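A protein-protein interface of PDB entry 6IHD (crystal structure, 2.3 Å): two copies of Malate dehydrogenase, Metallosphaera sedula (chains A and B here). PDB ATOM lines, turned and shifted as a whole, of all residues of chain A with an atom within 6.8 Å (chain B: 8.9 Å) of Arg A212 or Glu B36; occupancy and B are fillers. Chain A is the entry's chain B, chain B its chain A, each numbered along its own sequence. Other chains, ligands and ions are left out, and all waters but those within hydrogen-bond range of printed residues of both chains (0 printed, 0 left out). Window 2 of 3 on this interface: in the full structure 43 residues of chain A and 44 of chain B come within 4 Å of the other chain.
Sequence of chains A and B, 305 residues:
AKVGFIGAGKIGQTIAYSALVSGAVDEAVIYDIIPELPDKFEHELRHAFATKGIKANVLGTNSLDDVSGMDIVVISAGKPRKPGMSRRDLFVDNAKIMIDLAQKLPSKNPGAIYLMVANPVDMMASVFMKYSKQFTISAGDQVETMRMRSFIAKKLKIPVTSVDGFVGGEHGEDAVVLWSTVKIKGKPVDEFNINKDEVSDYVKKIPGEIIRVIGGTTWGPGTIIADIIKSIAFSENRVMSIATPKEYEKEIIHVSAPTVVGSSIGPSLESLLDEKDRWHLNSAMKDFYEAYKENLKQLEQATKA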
ATOM      1  N   PRO A  83       9.206 -12.575  29.789  1.00  0.00           N
ATOM      2  CA  PRO A  83       7.798 -12.401  29.307  1.00  0.00           C
ATOM      3  C   PRO A  83       7.250 -13.595  28.502  1.00  0.00           C
ATOM      4  O   PRO A  83       7.966 -14.140  27.669  1.00  0.00           O
ATOM      5  CB  PRO A  83       7.858 -11.144  28.415  1.00  0.00           C
ATOM      6  CG  PRO A  83       9.227 -10.585  28.552  1.00  0.00           C
ATOM      7  CD  PRO A  83       9.975 -11.325  29.625  1.00  0.00           C
ATOM      8  N   PRO A 207      11.399  -3.356  32.822  1.00  0.00           N
ATOM      9  CA  PRO A 207      12.273  -4.526  33.005  1.00  0.00           C
ATOM     10  C   PRO A 207      12.197  -5.509  31.860  1.00  0.00           C
ATOM     11  O   PRO A 207      13.244  -6.052  31.463  1.00  0.00           O
ATOM     12  CB  PRO A 207      11.817  -5.170  34.340  1.00  0.00           C
ATOM     13  CG  PRO A 207      10.585  -4.457  34.759  1.00  0.00           C
ATOM     14  CD  PRO A 207      10.369  -3.263  33.885  1.00  0.00           C
ATOM     15  N   GLY A 208      10.993  -5.710  31.326  1.00  0.00           N
ATOM     16  CA  GLY A 208      10.784  -6.538  30.101  1.00  0.00           C
ATOM     17  C   GLY A 208      11.532  -6.064  28.862  1.00  0.00           C
ATOM     18  O   GLY A 208      12.221  -6.852  28.186  1.00  0.00           O
ATOM     19  N   GLU A 209      11.403  -4.772  28.556  1.00  0.00           N
ATOM     20  CA  GLU A 209      12.241  -4.147  27.513  1.00  0.00           C
ATOM     21  C   GLU A 209      13.728  -4.426  27.737  1.00  0.00           C
ATOM     22  O   GLU A 209      14.423  -4.898  26.838  1.00  0.00           O
ATOM     23  CB  GLU A 209      11.942  -2.656  27.407  1.00  0.00           C
ATOM     24  CG  GLU A 209      10.503  -2.341  26.976  1.00  0.00           C
ATOM     25  CD  GLU A 209      10.066  -3.205  25.779  1.00  0.00           C
ATOM     26  OE1 GLU A 209       9.401  -4.232  25.983  1.00  0.00           O
ATOM     27  OE2 GLU A 209      10.445  -2.906  24.630  1.00  0.00           O
ATOM     28  N   ILE A 210      14.218  -4.278  28.957  1.00  0.00           N
ATOM     29  CA  ILE A 210      15.653  -4.461  29.198  1.00  0.00           C
ATOM     30  C   ILE A 210      16.101  -5.904  28.990  1.00  0.00           C
ATOM     31  O   ILE A 210      17.224  -6.150  28.527  1.00  0.00           O
ATOM     32  CB  ILE A 210      16.042  -3.981  30.612  1.00  0.00           C
ATOM     33  CG1 ILE A 210      15.926  -2.465  30.684  1.00  0.00           C
ATOM     34  CG2 ILE A 210      17.475  -4.391  30.998  1.00  0.00           C
ATOM     35  CD1 ILE A 210      15.861  -1.936  32.116  1.00  0.00           C
ATOM     36  N   ILE A 211      15.263  -6.841  29.413  1.00  0.00           N
ATOM     37  CA  ILE A 211      15.541  -8.257  29.279  1.00  0.00           C
ATOM     38  C   ILE A 211      15.524  -8.644  27.802  1.00  0.00           C
ATOM     39  O   ILE A 211      16.438  -9.321  27.318  1.00  0.00           O
ATOM     40  CB  ILE A 211      14.522  -9.103  30.094  1.00  0.00           C
ATOM     41  CG1 ILE A 211      14.777  -8.860  31.602  1.00  0.00           C
ATOM     42  CG2 ILE A 211      14.657 -10.613  29.773  1.00  0.00           C
ATOM     43  CD1 ILE A 211      13.627  -9.142  32.502  1.00  0.00           C
ATOM     44  N   ARG A 212      14.516  -8.181  27.084  1.00  0.00           N
ATOM     45  CA  ARG A 212      14.442  -8.417  25.658  1.00  0.00           C
ATOM     46  C   ARG A 212      15.760  -8.022  24.928  1.00  0.00           C
ATOM     47  O   ARG A 212      16.296  -8.800  24.165  1.00  0.00           O
ATOM     48  CB  ARG A 212      13.253  -7.650  25.078  1.00  0.00           C
ATOM     49  CG  ARG A 212      13.048  -7.914  23.610  1.00  0.00           C
ATOM     50  CD  ARG A 212      11.826  -7.217  23.031  1.00  0.00           C
ATOM     51  NE  ARG A 212      11.777  -5.791  23.289  1.00  0.00           N
ATOM     52  CZ  ARG A 212      12.532  -4.890  22.687  1.00  0.00           C
ATOM     53  NH1 ARG A 212      13.460  -5.261  21.812  1.00  0.00           N
ATOM     54  NH2 ARG A 212      12.396  -3.598  22.994  1.00  0.00           N
ATOM     55  N   VAL A 213      16.273  -6.826  25.185  1.00  0.00           N
ATOM     56  CA  VAL A 213      17.398  -6.316  24.431  1.00  0.00           C
ATOM     57  C   VAL A 213      18.670  -6.896  24.967  1.00  0.00           C
ATOM     58  O   VAL A 213      19.485  -7.370  24.196  1.00  0.00           O
ATOM     59  CB  VAL A 213      17.451  -4.784  24.472  1.00  0.00           C
ATOM     60  CG1 VAL A 213      18.751  -4.253  23.817  1.00  0.00           C
ATOM     61  CG2 VAL A 213      16.194  -4.223  23.810  1.00  0.00           C
ATOM     62  N   ILE A 214      18.837  -6.921  26.283  1.00  0.00           N
ATOM     63  CA  ILE A 214      20.130  -7.307  26.906  1.00  0.00           C
ATOM     64  C   ILE A 214      20.140  -8.748  27.404  1.00  0.00           C
ATOM     65  O   ILE A 214      21.173  -9.305  27.499  1.00  0.00           O
ATOM     66  CB  ILE A 214      20.567  -6.301  28.026  1.00  0.00           C
ATOM     67  CG1 ILE A 214      20.655  -4.913  27.405  1.00  0.00           C
ATOM     68  CG2 ILE A 214      21.914  -6.685  28.652  1.00  0.00           C
ATOM     69  CD1 ILE A 214      20.950  -3.756  28.314  1.00  0.00           C
ATOM     70  N   GLY A 215      19.010  -9.355  27.704  1.00  0.00           N
ATOM     71  CA  GLY A 215      19.005 -10.724  28.242  1.00  0.00           C
ATOM     72  C   GLY A 215      18.834 -10.818  29.752  1.00  0.00           C
ATOM     73  O   GLY A 215      18.665 -11.906  30.288  1.00  0.00           O
ATOM     74  N   GLY A 216      18.845  -9.683  30.442  1.00  0.00           N
ATOM     75  CA  GLY A 216      18.779  -9.676  31.891  1.00  0.00           C
ATOM     76  C   GLY A 216      18.947  -8.293  32.472  1.00  0.00           C
ATOM     77  O   GLY A 216      19.492  -7.379  31.832  1.00  0.00           O
ATOM     78  N   ALA B   8      29.581  -1.062  24.429  1.00  0.00           N
ATOM     79  CA  ALA B   8      28.725  -1.197  25.570  1.00  0.00           C
ATOM     80  C   ALA B   8      28.422  -2.687  25.797  1.00  0.00           C
ATOM     81  O   ALA B   8      27.270  -3.023  26.074  1.00  0.00           O
ATOM     82  CB  ALA B   8      27.404  -0.465  25.298  1.00  0.00           C
ATOM     83  N   ILE B  30      27.331   6.811  25.474  1.00  0.00           N
ATOM     84  CA  ILE B  30      27.631   5.403  25.300  1.00  0.00           C
ATOM     85  C   ILE B  30      27.064   4.863  23.986  1.00  0.00           C
ATOM     86  O   ILE B  30      25.855   4.984  23.706  1.00  0.00           O
ATOM     87  CB  ILE B  30      27.021   4.586  26.460  1.00  0.00           C
ATOM     88  CG1 ILE B  30      27.545   5.124  27.799  1.00  0.00           C
ATOM     89  CG2 ILE B  30      27.328   3.094  26.257  1.00  0.00           C
ATOM     90  CD1 ILE B  30      26.563   4.859  28.915  1.00  0.00           C
ATOM     91  N   ASP B  32      27.147   1.725  20.860  1.00  0.00           N
ATOM     92  CA  ASP B  32      27.361   0.350  20.412  1.00  0.00           C
ATOM     93  C   ASP B  32      26.615   0.203  19.089  1.00  0.00           C
ATOM     94  O   ASP B  32      25.659   0.921  18.820  1.00  0.00           O
ATOM     95  CB  ASP B  32      26.835  -0.653  21.456  1.00  0.00           C
ATOM     96  CG  ASP B  32      27.487  -2.057  21.316  1.00  0.00           C
ATOM     97  OD1 ASP B  32      27.077  -2.818  20.361  1.00  0.00           O
ATOM     98  OD2 ASP B  32      28.416  -2.391  22.148  1.00  0.00           O
ATOM     99  N   ILE B  33      27.055  -0.716  18.259  1.00  0.00           N
ATOM    100  CA  ILE B  33      26.290  -1.029  17.030  1.00  0.00           C
ATOM    101  C   ILE B  33      25.037  -1.871  17.301  1.00  0.00           C
ATOM    102  O   ILE B  33      24.129  -1.813  16.463  1.00  0.00           O
ATOM    103  CB  ILE B  33      27.151  -1.715  15.962  1.00  0.00           C
ATOM    104  CG1 ILE B  33      27.608  -3.125  16.459  1.00  0.00           C
ATOM    105  CG2 ILE B  33      28.363  -0.832  15.609  1.00  0.00           C
ATOM    106  CD1 ILE B  33      28.484  -3.891  15.502  1.00  0.00           C
ATOM    107  N   ILE B  34      24.950  -2.630  18.425  1.00  0.00           N
ATOM    108  CA  ILE B  34      23.753  -3.496  18.675  1.00  0.00           C
ATOM    109  C   ILE B  34      22.534  -2.632  18.922  1.00  0.00           C
ATOM    110  O   ILE B  34      22.572  -1.789  19.765  1.00  0.00           O
ATOM    111  CB  ILE B  34      23.861  -4.481  19.852  1.00  0.00           C
ATOM    112  CG1 ILE B  34      24.924  -5.532  19.518  1.00  0.00           C
ATOM    113  CG2 ILE B  34      22.465  -5.121  20.147  1.00  0.00           C
ATOM    114  CD1 ILE B  34      25.538  -6.274  20.691  1.00  0.00           C
ATOM    115  N   PRO B  35      21.464  -2.808  18.134  1.00  0.00           N
ATOM    116  CA  PRO B  35      20.386  -1.815  18.264  1.00  0.00           C
ATOM    117  C   PRO B  35      19.748  -1.801  19.641  1.00  0.00           C
ATOM    118  O   PRO B  35      19.554  -2.897  20.215  1.00  0.00           O
ATOM    119  CB  PRO B  35      19.381  -2.290  17.239  1.00  0.00           C
ATOM    120  CG  PRO B  35      20.176  -3.000  16.192  1.00  0.00           C
ATOM    121  CD  PRO B  35      21.439  -3.502  16.823  1.00  0.00           C
ATOM    122  N   GLU B  36      19.440  -0.608  20.181  1.00  0.00           N
ATOM    123  CA  GLU B  36      18.757  -0.489  21.489  1.00  0.00           C
ATOM    124  C   GLU B  36      19.510  -1.027  22.749  1.00  0.00           C
ATOM    125  O   GLU B  36      18.927  -1.072  23.837  1.00  0.00           O
ATOM    126  CB  GLU B  36      17.481  -1.356  21.561  1.00  0.00           C
ATOM    127  CG  GLU B  36      16.474  -1.233  20.458  1.00  0.00           C
ATOM    128  CD  GLU B  36      15.157  -1.837  20.907  1.00  0.00           C
ATOM    129  OE1 GLU B  36      14.433  -1.141  21.663  1.00  0.00           O
ATOM    130  OE2 GLU B  36      14.859  -3.002  20.549  1.00  0.00           O
ATOM    131  N   LEU B  37      20.738  -1.519  22.619  1.00  0.00           N
ATOM    132  CA  LEU B  37      21.499  -1.881  23.800  1.00  0.00           C
ATOM    133  C   LEU B  37      21.890  -0.599  24.630  1.00  0.00           C
ATOM    134  O   LEU B  37      21.622  -0.565  25.820  1.00  0.00           O
ATOM    135  CB  LEU B  37      22.713  -2.634  23.385  1.00  0.00           C
ATOM    136  CG  LEU B  37      23.793  -2.932  24.404  1.00  0.00           C
ATOM    137  CD1 LEU B  37      23.253  -3.925  25.389  1.00  0.00           C
ATOM    138  CD2 LEU B  37      24.968  -3.590  23.691  1.00  0.00           C
ATOM    139  N   PRO B  38      22.480   0.442  24.004  1.00  0.00           N
ATOM    140  CA  PRO B  38      22.839   1.600  24.817  1.00  0.00           C
ATOM    141  C   PRO B  38      21.655   2.261  25.485  1.00  0.00           C
ATOM    142  O   PRO B  38      21.766   2.713  26.599  1.00  0.00           O
ATOM    143  CB  PRO B  38      23.508   2.566  23.800  1.00  0.00           C
ATOM    144  CG  PRO B  38      24.100   1.609  22.783  1.00  0.00           C
ATOM    145  CD  PRO B  38      23.056   0.528  22.645  1.00  0.00           C
ATOM    146  N   ASP B  39      20.542   2.329  24.798  1.00  0.00           N
ATOM    147  CA  ASP B  39      19.293   2.856  25.349  1.00  0.00           C
ATOM    148  C   ASP B  39      18.933   2.118  26.634  1.00  0.00           C
ATOM    149  O   ASP B  39      18.656   2.746  27.671  1.00  0.00           O
ATOM    150  CB  ASP B  39      18.132   2.704  24.334  1.00  0.00           C
ATOM    151  CG  ASP B  39      16.827   3.310  24.831  1.00  0.00           C
ATOM    152  OD1 ASP B  39      16.777   4.512  25.048  1.00  0.00           O
ATOM    153  OD2 ASP B  39      15.824   2.602  24.974  1.00  0.00           O
ATOM    154  N   LYS B  40      18.981   0.799  26.579  1.00  0.00           N
ATOM    155  CA  LYS B  40      18.559  -0.026  27.741  1.00  0.00           C
ATOM    156  C   LYS B  40      19.578  -0.004  28.886  1.00  0.00           C
ATOM    157  O   LYS B  40      19.192   0.070  30.058  1.00  0.00           O
ATOM    158  CB  LYS B  40      18.267  -1.464  27.305  1.00  0.00           C
ATOM    159  CG  LYS B  40      16.798  -1.660  26.946  1.00  0.00           C
ATOM    160  CD  LYS B  40      16.366  -0.752  25.822  1.00  0.00           C
ATOM    161  CE  LYS B  40      14.875  -0.829  25.637  1.00  0.00           C
ATOM    162  NZ  LYS B  40      14.507  -0.118  24.392  1.00  0.00           N
ATOM    163  N   PHE B  41      20.867  -0.027  28.531  1.00  0.00           N
ATOM    164  CA  PHE B  41      21.935   0.211  29.476  1.00  0.00           C
ATOM    165  C   PHE B  41      21.789   1.564  30.150  1.00  0.00           C
ATOM    166  O   PHE B  41      21.935   1.642  31.339  1.00  0.00           O
ATOM    167  CB  PHE B  41      23.301   0.142  28.802  1.00  0.00           C
ATOM    168  CG  PHE B  41      24.460   0.361  29.752  1.00  0.00           C
ATOM    169  CD1 PHE B  41      24.554  -0.370  30.950  1.00  0.00           C
ATOM    170  CD2 PHE B  41      25.505   1.244  29.421  1.00  0.00           C
ATOM    171  CE1 PHE B  41      25.642  -0.218  31.789  1.00  0.00           C
ATOM    172  CE2 PHE B  41      26.586   1.427  30.276  1.00  0.00           C
ATOM    173  CZ  PHE B  41      26.633   0.732  31.475  1.00  0.00           C
ATOM    174  N   GLU B  42      21.508   2.620  29.386  1.00  0.00           N
ATOM    175  CA  GLU B  42      21.227   3.960  29.979  1.00  0.00           C
ATOM    176  C   GLU B  42      20.067   3.883  30.970  1.00  0.00           C
ATOM    177  O   GLU B  42      20.083   4.547  31.991  1.00  0.00           O
ATOM    178  CB  GLU B  42      20.928   5.009  28.913  1.00  0.00           C
ATOM    179  CG  GLU B  42      20.662   6.401  29.449  1.00  0.00           C
ATOM    180  CD  GLU B  42      19.942   7.360  28.484  1.00  0.00           C
ATOM    181  OE1 GLU B  42      20.342   7.489  27.278  1.00  0.00           O
ATOM    182  OE2 GLU B  42      18.975   8.017  28.964  1.00  0.00           O
ATOM    183  N   HIS B  43      19.062   3.086  30.669  1.00  0.00           N
ATOM    184  CA  HIS B  43      17.922   2.937  31.612  1.00  0.00           C
ATOM    185  C   HIS B  43      18.350   2.329  32.957  1.00  0.00           C
ATOM    186  O   HIS B  43      17.910   2.839  34.031  1.00  0.00           O
ATOM    187  CB  HIS B  43      16.769   2.115  31.018  1.00  0.00           C
ATOM    188  CG  HIS B  43      15.834   2.953  30.240  1.00  0.00           C
ATOM    189  ND1 HIS B  43      14.823   3.678  30.840  1.00  0.00           N
ATOM    190  CD2 HIS B  43      15.793   3.260  28.929  1.00  0.00           C
ATOM    191  CE1 HIS B  43      14.194   4.390  29.927  1.00  0.00           C
ATOM    192  NE2 HIS B  43      14.739   4.126  28.757  1.00  0.00           N
ATOM    193  N   GLY B  60      22.656   6.949  26.041  1.00  0.00           N
ATOM    194  CA  GLY B  60      22.842   5.734  25.225  1.00  0.00           C
ATOM    195  C   GLY B  60      22.452   6.018  23.779  1.00  0.00           C
ATOM    196  O   GLY B  60      21.423   6.600  23.532  1.00  0.00           O
ATOM    197  N   THR B  61      23.305   5.654  22.823  1.00  0.00           N
ATOM    198  CA  THR B  61      23.047   5.978  21.435  1.00  0.00           C
ATOM    199  C   THR B  61      23.466   4.872  20.494  1.00  0.00           C
ATOM    200  O   THR B  61      24.468   4.158  20.747  1.00  0.00           O
ATOM    201  CB  THR B  61      23.737   7.328  21.105  1.00  0.00           C
ATOM    202  OG1 THR B  61      23.233   7.864  19.880  1.00  0.00           O
ATOM    203  CG2 THR B  61      25.269   7.190  21.059  1.00  0.00           C
ATOM    204  N   ASN B  62      22.698   4.713  19.409  1.00  0.00           N
ATOM    205  CA  ASN B  62      23.119   3.857  18.296  1.00  0.00           C
ATOM    206  C   ASN B  62      23.694   4.733  17.122  1.00  0.00           C
ATOM    207  O   ASN B  62      23.979   4.213  16.022  1.00  0.00           O
ATOM    208  CB  ASN B  62      21.975   2.965  17.830  1.00  0.00           C
ATOM    209  CG  ASN B  62      21.759   1.724  18.691  1.00  0.00           C
ATOM    210  OD1 ASN B  62      20.656   1.507  19.192  1.00  0.00           O
ATOM    211  ND2 ASN B  62      22.782   0.896  18.832  1.00  0.00           N
ATOM    212  N   SER B  63      23.888   6.033  17.368  1.00  0.00           N
ATOM    213  CA  SER B  63      24.504   6.958  16.398  1.00  0.00           C
ATOM    214  C   SER B  63      25.817   7.476  16.936  1.00  0.00           C
ATOM    215  O   SER B  63      25.857   8.360  17.804  1.00  0.00           O
ATOM    216  CB  SER B  63      23.587   8.140  16.174  1.00  0.00           C
ATOM    217  OG  SER B  63      24.210   9.151  15.412  1.00  0.00           O
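The side-chain carboxylate (OE2) of Glu B36 lies within salt-bridge range of the guanidinium group (NH1) of Arg A212 (2.9 Å).
The side-chain carboxylate (OE2) of Glu A209 is in salt-bridge range of the guanidinium group (NH2) of Arg A212, 2.6 Å away. OE1 of Glu B36 is in salt-bridge range of NZ of Lys B40. The side-chain carboxylate of Asp B39 lies within salt-bridge range of the side-chain amino group of Lys B40 (3.1 Å). The side-chain amide oxygen of Asn B62 lies within hydrogen-bond range of the backbone NH of Glu B36 (2.6 Å).
Glu A209 touches Lys B40 (CB to CE, 3.9 Å). CG of Lys B40 touches CA of Ile A210, 3.8 Å away. Pro B35 touches Val A213 (O to CG1, 3.9 Å). O of Glu B36 touches CG1 of Val A213, at 3.2 Å. Leu B37 touches Val A213 (N to CG1, 3.6 Å). Leu B37 touches Ile A214 (CD1 to CG1, 3.4 Å). CD1 of Ile A214 touches CB of Lys B40, at 3.7 Å. N of Phe B41 touches CD1 of Ile A214, 3.7 Å away.
Of chain B, only Glu B36 (2.9 Å) comes within 4 Å of Arg A212. Of chain A, only Arg A212 and Val A213 come within 4 Å of Glu B36. Of the printed residues of chain B, Glu A209 touches Lys B40. Of the printed residues of chain B, Ile A214 touches Leu B37 (3.4 Å), Lys B40 (3.7 Å) and Phe B41 (3.7 Å). Of the printed residues of chain B, Ile A210 touches Lys B40 (3.8 Å). Of the printed residues of chain B, Val A213 touches Pro B35 (3.9 Å), Glu B36 (3.2 Å) and Leu B37 (3.6 Å). The nearest residue of chain A that does not touch Glu B36 is Glu A209 (5.3 Å). The nearest printed residue of chain B that does not touch Val A213 is Lys B40 (4.02 Å).
Of the 18 printed residues of chain B, 5 touch a printed residue of chain A. Hydrophobic or aromatic side chains of chain B within 4 Å of the printed part of chain A: Leu B37. Of the 11 printed residues of chain A, 5 touch a printed residue of chain B.
No position is printed for both chains.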
